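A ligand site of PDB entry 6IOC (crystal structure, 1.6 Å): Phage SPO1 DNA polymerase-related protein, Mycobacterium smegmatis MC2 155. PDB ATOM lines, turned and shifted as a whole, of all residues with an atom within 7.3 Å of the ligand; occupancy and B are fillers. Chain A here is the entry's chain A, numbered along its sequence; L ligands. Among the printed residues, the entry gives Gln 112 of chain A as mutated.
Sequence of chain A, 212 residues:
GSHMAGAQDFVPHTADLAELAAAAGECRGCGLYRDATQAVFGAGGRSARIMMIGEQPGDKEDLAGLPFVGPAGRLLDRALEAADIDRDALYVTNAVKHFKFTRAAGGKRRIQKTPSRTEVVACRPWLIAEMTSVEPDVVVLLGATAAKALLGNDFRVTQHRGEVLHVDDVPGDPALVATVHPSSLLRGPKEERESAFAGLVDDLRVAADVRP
The side-chain amide oxygen (OD1) of Asn 94 lies within hydrogen-bond range of a nitrogen (N2) of the ligand (2.7 Å).
O1 of the ligand is in hydrogen-bond range of NE2 of His 181.
N of Gln 56 is in hydrogen-bond range of O1 of the ligand (3.2 Å).
The side-chain amide nitrogen of Gln 112 sits close to a nitrogen (N1) of the ligand (3.1 Å).
The backbone NH (N) of Glu 55 is in hydrogen-bond range of an oxygen (O1) of the ligand (2.7 Å).
The backbone NH (N) of Phe 68 sits at hydrogen-bond distance from an oxygen (O2) of the ligand.
The backbone carbonyl oxygen (O) of Gln 56 is in hydrogen-bond range of a nitrogen (N2) of the ligand (2.8 Å).
The backbone NH (N) of Ala 95 is in hydrogen-bond range of the backbone carbonyl oxygen (O) of Glu 55, 3.4 Å away.
O of Thr 93 is in hydrogen-bond range of N of Gly 54 (2.8 Å).
The backbone carbonyl oxygen of Gly 54 lies within hydrogen-bond range of the backbone NH of Ala 95 (2.9 Å).
O of Glu 55 is in hydrogen-bond range of N of Val 96, at 3.1 Å.
OE2 of Glu 61 lies within hydrogen-bond range of N of Val 69.
OE2 of Glu 61 sits at hydrogen-bond distance from N of Gly 70, at 2.9 Å.
The backbone NH of Phe 68 lies close to the side-chain carboxylate of Glu 61 (3.5 Å).
ND1 of His 181 lies within hydrogen-bond range of N of Ser 183 (2.8 Å).
Gly 54 touches the ligand (C to O1, 3.7 Å).
Gly 58 touches the ligand.
Glu 61 touches the ligand (OE2 to C3, 3.2 Å).
Pro 67 touches the ligand (CA to O2, 3.3 Å).
CB of Ala 72 touches C4 of the ligand, at 3.9 Å.
OG of Ser 183 touches N1 of the ligand, at 3.9 Å.
The nearest printed residue that does not touch the ligand is Pro 57 (4.1 Å).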
ATOM      1  N   VAL A  40       6.536  33.836  -7.193  1.00  0.00           N
ATOM      2  CA  VAL A  40       7.242  32.792  -6.461  1.00  0.00           C
ATOM      3  C   VAL A  40       8.628  32.691  -7.085  1.00  0.00           C
ATOM      4  O   VAL A  40       8.786  32.188  -8.200  1.00  0.00           O
ATOM      5  CB  VAL A  40       6.509  31.453  -6.534  1.00  0.00           C
ATOM      6  CG1 VAL A  40       7.307  30.351  -5.837  1.00  0.00           C
ATOM      7  CG2 VAL A  40       5.116  31.597  -5.883  1.00  0.00           C
ATOM      8  N   ILE A  53      14.616  23.375 -12.075  1.00  0.00           N
ATOM      9  CA  ILE A  53      13.599  24.288 -12.602  1.00  0.00           C
ATOM     10  C   ILE A  53      12.330  23.499 -12.876  1.00  0.00           C
ATOM     11  O   ILE A  53      12.341  22.602 -13.732  1.00  0.00           O
ATOM     12  CB  ILE A  53      14.051  24.988 -13.891  1.00  0.00           C
ATOM     13  CG1 ILE A  53      15.405  25.674 -13.682  1.00  0.00           C
ATOM     14  CG2 ILE A  53      12.977  25.965 -14.324  1.00  0.00           C
ATOM     15  CD1 ILE A  53      15.974  26.302 -14.977  1.00  0.00           C
ATOM     16  N   GLY A  54      11.258  23.836 -12.172  1.00  0.00           N
ATOM     17  CA  GLY A  54       9.944  23.267 -12.426  1.00  0.00           C
ATOM     18  C   GLY A  54       9.148  24.106 -13.393  1.00  0.00           C
ATOM     19  O   GLY A  54       9.697  24.944 -14.110  1.00  0.00           O
ATOM     20  N   GLU A  55       7.822  23.895 -13.418  1.00  0.00           N
ATOM     21  CA  GLU A  55       6.968  24.563 -14.380  1.00  0.00           C
ATOM     22  C   GLU A  55       6.478  25.922 -13.858  1.00  0.00           C
ATOM     23  O   GLU A  55       6.701  26.956 -14.486  1.00  0.00           O
ATOM     24  CB  GLU A  55       5.760  23.702 -14.754  1.00  0.00           C
ATOM     25  CG  GLU A  55       4.875  24.390 -15.807  1.00  0.00           C
ATOM     26  CD  GLU A  55       3.676  23.558 -16.229  1.00  0.00           C
ATOM     27  OE1 GLU A  55       3.747  22.885 -17.288  1.00  0.00           O
ATOM     28  OE2 GLU A  55       2.665  23.576 -15.497  1.00  0.00           O
ATOM     29  N   GLN A  56       5.790  25.913 -12.726  1.00  0.00           N
ATOM     30  CA  GLN A  56       5.181  27.142 -12.211  1.00  0.00           C
ATOM     31  C   GLN A  56       4.742  26.838 -10.779  1.00  0.00           C
ATOM     32  O   GLN A  56       4.630  25.662 -10.422  1.00  0.00           O
ATOM     33  CB  GLN A  56       3.987  27.547 -13.066  1.00  0.00           C
ATOM     34  CG  GLN A  56       2.863  26.538 -12.833  1.00  0.00           C
ATOM     35  CD  GLN A  56       1.616  26.952 -13.473  1.00  0.00           C
ATOM     36  OE1 GLN A  56       1.098  28.038 -13.187  1.00  0.00           O
ATOM     37  NE2 GLN A  56       1.086  26.096 -14.376  1.00  0.00           N
ATOM     38  N   PRO A  57       4.448  27.840  -9.969  1.00  0.00           N
ATOM     39  CA  PRO A  57       3.896  27.536  -8.638  1.00  0.00           C
ATOM     40  C   PRO A  57       2.532  26.878  -8.770  1.00  0.00           C
ATOM     41  O   PRO A  57       1.809  27.070  -9.743  1.00  0.00           O
ATOM     42  CB  PRO A  57       3.748  28.918  -7.970  1.00  0.00           C
ATOM     43  CG  PRO A  57       4.280  29.932  -8.933  1.00  0.00           C
ATOM     44  CD  PRO A  57       4.407  29.271 -10.281  1.00  0.00           C
ATOM     45  N   GLY A  58       2.189  26.078  -7.773  1.00  0.00           N
ATOM     46  CA  GLY A  58       0.831  25.620  -7.602  1.00  0.00           C
ATOM     47  C   GLY A  58       0.111  26.408  -6.535  1.00  0.00           C
ATOM     48  O   GLY A  58       0.572  27.459  -6.074  1.00  0.00           O
ATOM     49  N   ASP A  59      -1.028  25.862  -6.087  1.00  0.00           N
ATOM     50  CA  ASP A  59      -1.899  26.546  -5.141  1.00  0.00           C
ATOM     51  C   ASP A  59      -1.157  26.969  -3.864  1.00  0.00           C
ATOM     52  O   ASP A  59      -1.090  28.170  -3.505  1.00  0.00           O
ATOM     53  CB  ASP A  59      -3.066  25.562  -4.875  1.00  0.00           C
ATOM     54  CG  ASP A  59      -4.041  26.041  -3.820  1.00  0.00           C
ATOM     55  OD1 ASP A  59      -4.178  27.257  -3.590  1.00  0.00           O
ATOM     56  OD2 ASP A  59      -4.682  25.145  -3.222  1.00  0.00           O
ATOM     57  N   GLU A  61       2.067  26.965  -3.250  1.00  0.00           N
ATOM     58  CA  GLU A  61       3.216  27.800  -3.589  1.00  0.00           C
ATOM     59  C   GLU A  61       2.829  29.263  -3.683  1.00  0.00           C
ATOM     60  O   GLU A  61       3.551  30.152  -3.200  1.00  0.00           O
ATOM     61  CB  GLU A  61       3.808  27.336  -4.905  1.00  0.00           C
ATOM     62  CG  GLU A  61       4.609  26.021  -4.857  1.00  0.00           C
ATOM     63  CD  GLU A  61       3.738  24.771  -4.772  1.00  0.00           C
ATOM     64  OE1 GLU A  61       2.534  24.828  -5.111  1.00  0.00           O
ATOM     65  OE2 GLU A  61       4.269  23.694  -4.412  1.00  0.00           O
ATOM     66  N   LEU A  66       6.893  30.347  -2.098  1.00  0.00           N
ATOM     67  CA  LEU A  66       8.057  29.468  -2.231  1.00  0.00           C
ATOM     68  C   LEU A  66       7.709  28.302  -3.146  1.00  0.00           C
ATOM     69  O   LEU A  66       6.556  27.832  -3.151  1.00  0.00           O
ATOM     70  CB  LEU A  66       8.463  28.889  -0.868  1.00  0.00           C
ATOM     71  CG  LEU A  66       8.911  29.878   0.182  1.00  0.00           C
ATOM     72  CD1 LEU A  66       8.813  29.219   1.532  1.00  0.00           C
ATOM     73  CD2 LEU A  66      10.338  30.240  -0.135  1.00  0.00           C
ATOM     74  N   PRO A  67       8.673  27.776  -3.897  1.00  0.00           N
ATOM     75  CA  PRO A  67       8.373  26.689  -4.840  1.00  0.00           C
ATOM     76  C   PRO A  67       8.374  25.332  -4.154  1.00  0.00           C
ATOM     77  O   PRO A  67       9.012  25.123  -3.132  1.00  0.00           O
ATOM     78  CB  PRO A  67       9.502  26.776  -5.867  1.00  0.00           C
ATOM     79  CG  PRO A  67      10.663  27.304  -5.064  1.00  0.00           C
ATOM     80  CD  PRO A  67      10.067  28.281  -4.060  1.00  0.00           C
ATOM     81  N   PHE A  68       7.627  24.409  -4.772  1.00  0.00           N
ATOM     82  CA  PHE A  68       7.619  22.993  -4.400  1.00  0.00           C
ATOM     83  C   PHE A  68       7.337  22.781  -2.912  1.00  0.00           C
ATOM     84  O   PHE A  68       8.056  22.060  -2.211  1.00  0.00           O
ATOM     85  CB  PHE A  68       8.933  22.344  -4.819  1.00  0.00           C
ATOM     86  CG  PHE A  68       8.995  22.014  -6.297  1.00  0.00           C
ATOM     87  CD1 PHE A  68       8.258  20.967  -6.805  1.00  0.00           C
ATOM     88  CD2 PHE A  68       9.763  22.763  -7.169  1.00  0.00           C
ATOM     89  CE1 PHE A  68       8.286  20.662  -8.145  1.00  0.00           C
ATOM     90  CE2 PHE A  68       9.800  22.473  -8.523  1.00  0.00           C
ATOM     91  CZ  PHE A  68       9.076  21.402  -9.012  1.00  0.00           C
ATOM     92  N   VAL A  69       6.247  23.388  -2.420  1.00  0.00           N
ATOM     93  CA  VAL A  69       5.801  23.144  -1.049  1.00  0.00           C
ATOM     94  C   VAL A  69       4.544  22.301  -0.985  1.00  0.00           C
ATOM     95  O   VAL A  69       4.173  21.881   0.125  1.00  0.00           O
ATOM     96  CB  VAL A  69       5.599  24.461  -0.258  1.00  0.00           C
ATOM     97  CG1 VAL A  69       6.913  25.181  -0.110  1.00  0.00           C
ATOM     98  CG2 VAL A  69       4.528  25.354  -0.902  1.00  0.00           C
ATOM     99  N   GLY A  70       3.883  22.031  -2.100  1.00  0.00           N
ATOM    100  CA  GLY A  70       2.708  21.199  -2.127  1.00  0.00           C
ATOM    101  C   GLY A  70       3.039  19.746  -2.454  1.00  0.00           C
ATOM    102  O   GLY A  70       4.169  19.297  -2.207  1.00  0.00           O
ATOM    103  N   PRO A  71       2.071  19.016  -3.016  1.00  0.00           N
ATOM    104  CA  PRO A  71       2.277  17.578  -3.303  1.00  0.00           C
ATOM    105  C   PRO A  71       3.477  17.275  -4.193  1.00  0.00           C
ATOM    106  O   PRO A  71       4.211  16.299  -3.950  1.00  0.00           O
ATOM    107  CB  PRO A  71       0.978  17.168  -4.017  1.00  0.00           C
ATOM    108  CG  PRO A  71      -0.018  18.140  -3.574  1.00  0.00           C
ATOM    109  CD  PRO A  71       0.696  19.432  -3.300  1.00  0.00           C
ATOM    110  N   ALA A  72       3.637  18.058  -5.269  1.00  0.00           N
ATOM    111  CA  ALA A  72       4.786  17.870  -6.143  1.00  0.00           C
ATOM    112  C   ALA A  72       6.087  17.980  -5.385  1.00  0.00           C
ATOM    113  O   ALA A  72       7.029  17.252  -5.676  1.00  0.00           O
ATOM    114  CB  ALA A  72       4.780  18.895  -7.282  1.00  0.00           C
ATOM    115  N   GLY A  73       6.163  18.871  -4.382  1.00  0.00           N
ATOM    116  CA  GLY A  73       7.351  18.963  -3.553  1.00  0.00           C
ATOM    117  C   GLY A  73       7.580  17.721  -2.706  1.00  0.00           C
ATOM    118  O   GLY A  73       8.736  17.346  -2.458  1.00  0.00           O
ATOM    119  N   ARG A  87      18.159  18.928  -0.396  1.00  0.00           N
ATOM    120  CA  ARG A  87      17.393  20.002  -1.009  1.00  0.00           C
ATOM    121  C   ARG A  87      17.932  21.384  -0.629  1.00  0.00           C
ATOM    122  O   ARG A  87      17.879  22.318  -1.441  1.00  0.00           O
ATOM    123  CB  ARG A  87      15.923  19.894  -0.613  1.00  0.00           C
ATOM    124  CG  ARG A  87      15.069  21.004  -1.245  1.00  0.00           C
ATOM    125  CD  ARG A  87      13.621  20.616  -1.187  1.00  0.00           C
ATOM    126  NE  ARG A  87      12.771  21.744  -1.524  1.00  0.00           N
ATOM    127  CZ  ARG A  87      11.458  21.651  -1.708  1.00  0.00           C
ATOM    128  NH1 ARG A  87      10.846  20.474  -1.579  1.00  0.00           N
ATOM    129  NH2 ARG A  87      10.753  22.734  -2.005  1.00  0.00           N
ATOM    130  N   VAL A  92      16.272  25.962  -6.302  1.00  0.00           N
ATOM    131  CA  VAL A  92      15.049  25.443  -6.911  1.00  0.00           C
ATOM    132  C   VAL A  92      14.177  26.611  -7.375  1.00  0.00           C
ATOM    133  O   VAL A  92      13.871  27.514  -6.578  1.00  0.00           O
ATOM    134  CB  VAL A  92      14.284  24.575  -5.905  1.00  0.00           C
ATOM    135  CG1 VAL A  92      13.000  24.079  -6.522  1.00  0.00           C
ATOM    136  CG2 VAL A  92      15.203  23.407  -5.452  1.00  0.00           C
ATOM    137  N   THR A  93      13.772  26.614  -8.649  1.00  0.00           N
ATOM    138  CA  THR A  93      12.901  27.689  -9.147  1.00  0.00           C
ATOM    139  C   THR A  93      11.955  27.097 -10.187  1.00  0.00           C
ATOM    140  O   THR A  93      11.892  25.877 -10.337  1.00  0.00           O
ATOM    141  CB  THR A  93      13.752  28.848  -9.677  1.00  0.00           C
ATOM    142  OG1 THR A  93      12.954  30.025  -9.851  1.00  0.00           O
ATOM    143  CG2 THR A  93      14.462  28.493 -10.993  1.00  0.00           C
ATOM    144  N   ASN A  94      11.202  27.953 -10.890  1.00  0.00           N
ATOM    145  CA  ASN A  94      10.222  27.535 -11.899  1.00  0.00           C
ATOM    146  C   ASN A  94      10.382  28.378 -13.167  1.00  0.00           C
ATOM    147  O   ASN A  94      10.866  29.509 -13.131  1.00  0.00           O
ATOM    148  CB  ASN A  94       8.786  27.701 -11.396  1.00  0.00           C
ATOM    149  CG  ASN A  94       8.410  26.671 -10.375  1.00  0.00           C
ATOM    150  OD1 ASN A  94       8.543  25.479 -10.604  1.00  0.00           O
ATOM    151  ND2 ASN A  94       8.015  27.132  -9.182  1.00  0.00           N
ATOM    152  N   ALA A  95       9.966  27.792 -14.308  1.00  0.00           N
ATOM    153  CA  ALA A  95      10.041  28.514 -15.580  1.00  0.00           C
ATOM    154  C   ALA A  95       9.191  29.780 -15.556  1.00  0.00           C
ATOM    155  O   ALA A  95       9.571  30.810 -16.108  1.00  0.00           O
ATOM    156  CB  ALA A  95       9.586  27.599 -16.727  1.00  0.00           C
ATOM    157  N   VAL A  96       8.033  29.692 -14.909  1.00  0.00           N
ATOM    158  CA  VAL A  96       7.073  30.772 -14.817  1.00  0.00           C
ATOM    159  C   VAL A  96       6.901  31.104 -13.344  1.00  0.00           C
ATOM    160  O   VAL A  96       6.801  30.199 -12.504  1.00  0.00           O
ATOM    161  CB  VAL A  96       5.757  30.315 -15.498  1.00  0.00           C
ATOM    162  CG1 VAL A  96       4.586  31.152 -15.131  1.00  0.00           C
ATOM    163  CG2 VAL A  96       6.001  30.315 -17.004  1.00  0.00           C
ATOM    164  N   GLN A 112      -3.282  24.176 -11.296  1.00  0.00           N
ATOM    165  CA  GLN A 112      -2.441  24.688 -12.387  1.00  0.00           C
ATOM    166  C   GLN A 112      -3.065  24.454 -13.765  1.00  0.00           C
ATOM    167  O   GLN A 112      -3.644  23.395 -14.035  1.00  0.00           O
ATOM    168  CB  GLN A 112      -1.064  24.018 -12.301  1.00  0.00           C
ATOM    169  CG  GLN A 112      -0.286  24.395 -11.049  1.00  0.00           C
ATOM    170  CD  GLN A 112       0.795  23.389 -10.676  1.00  0.00           C
ATOM    171  OE1 GLN A 112       0.519  22.212 -10.477  1.00  0.00           O
ATOM    172  NE2 GLN A 112       2.038  23.868 -10.576  1.00  0.00           N
ATOM    173  N   LEU A 142      12.799  20.058 -14.885  1.00  0.00           N
ATOM    174  CA  LEU A 142      11.738  19.146 -14.476  1.00  0.00           C
ATOM    175  C   LEU A 142      10.507  19.348 -15.360  1.00  0.00           C
ATOM    176  O   LEU A 142       9.693  20.226 -15.099  1.00  0.00           O
ATOM    177  CB  LEU A 142      11.370  19.361 -13.012  1.00  0.00           C
ATOM    178  CG  LEU A 142      12.583  19.247 -12.112  1.00  0.00           C
ATOM    179  CD1 LEU A 142      12.231  19.808 -10.725  1.00  0.00           C
ATOM    180  CD2 LEU A 142      13.019  17.768 -12.025  1.00  0.00           C
ATOM    181  N   HIS A 181       8.682  15.666 -14.611  1.00  0.00           N
ATOM    182  CA  HIS A 181       8.241  16.580 -13.573  1.00  0.00           C
ATOM    183  C   HIS A 181       7.621  15.766 -12.452  1.00  0.00           C
ATOM    184  O   HIS A 181       6.807  14.901 -12.723  1.00  0.00           O
ATOM    185  CB  HIS A 181       7.177  17.544 -14.119  1.00  0.00           C
ATOM    186  CG  HIS A 181       6.840  18.662 -13.189  1.00  0.00           C
ATOM    187  ND1 HIS A 181       6.229  18.461 -11.966  1.00  0.00           N
ATOM    188  CD2 HIS A 181       7.014  20.003 -13.292  1.00  0.00           C
ATOM    189  CE1 HIS A 181       6.057  19.619 -11.361  1.00  0.00           C
ATOM    190  NE2 HIS A 181       6.519  20.571 -12.145  1.00  0.00           N
ATOM    191  N   PRO A 182       7.985  16.001 -11.178  1.00  0.00           N
ATOM    192  CA  PRO A 182       7.361  15.226 -10.090  1.00  0.00           C
ATOM    193  C   PRO A 182       5.834  15.247 -10.098  1.00  0.00           C
ATOM    194  O   PRO A 182       5.215  14.243  -9.738  1.00  0.00           O
ATOM    195  CB  PRO A 182       7.905  15.900  -8.817  1.00  0.00           C
ATOM    196  CG  PRO A 182       9.197  16.497  -9.226  1.00  0.00           C
ATOM    197  CD  PRO A 182       9.046  16.886 -10.684  1.00  0.00           C
ATOM    198  N   SER A 183       5.195  16.373 -10.469  1.00  0.00           N
ATOM    199  CA  SER A 183       3.725  16.397 -10.522  1.00  0.00           C
ATOM    200  C   SER A 183       3.163  15.365 -11.486  1.00  0.00           C
ATOM    201  O   SER A 183       2.035  14.900 -11.286  1.00  0.00           O
ATOM    202  CB  SER A 183       3.212  17.770 -10.945  1.00  0.00           C
ATOM    203  OG  SER A 183       3.377  18.715  -9.919  1.00  0.00           O
HETATM  204  N1  LIG L   1       4.691  22.406  -9.728  1.00  0.00           N
HETATM  205  C1  LIG L   1       5.870  23.136 -10.255  1.00  0.00           C
HETATM  206  O1  LIG L   1       6.212  23.010 -11.376  1.00  0.00           O
HETATM  207  N2  LIG L   1       6.652  24.060  -9.387  1.00  0.00           N
HETATM  208  C2  LIG L   1       6.276  24.286  -8.008  1.00  0.00           C
HETATM  209  O2  LIG L   1       6.907  25.054  -7.314  1.00  0.00           O
HETATM  210  C3  LIG L   1       5.080  23.550  -7.497  1.00  0.00           C
HETATM  211  C4  LIG L   1       4.342  22.636  -8.341  1.00  0.00           C
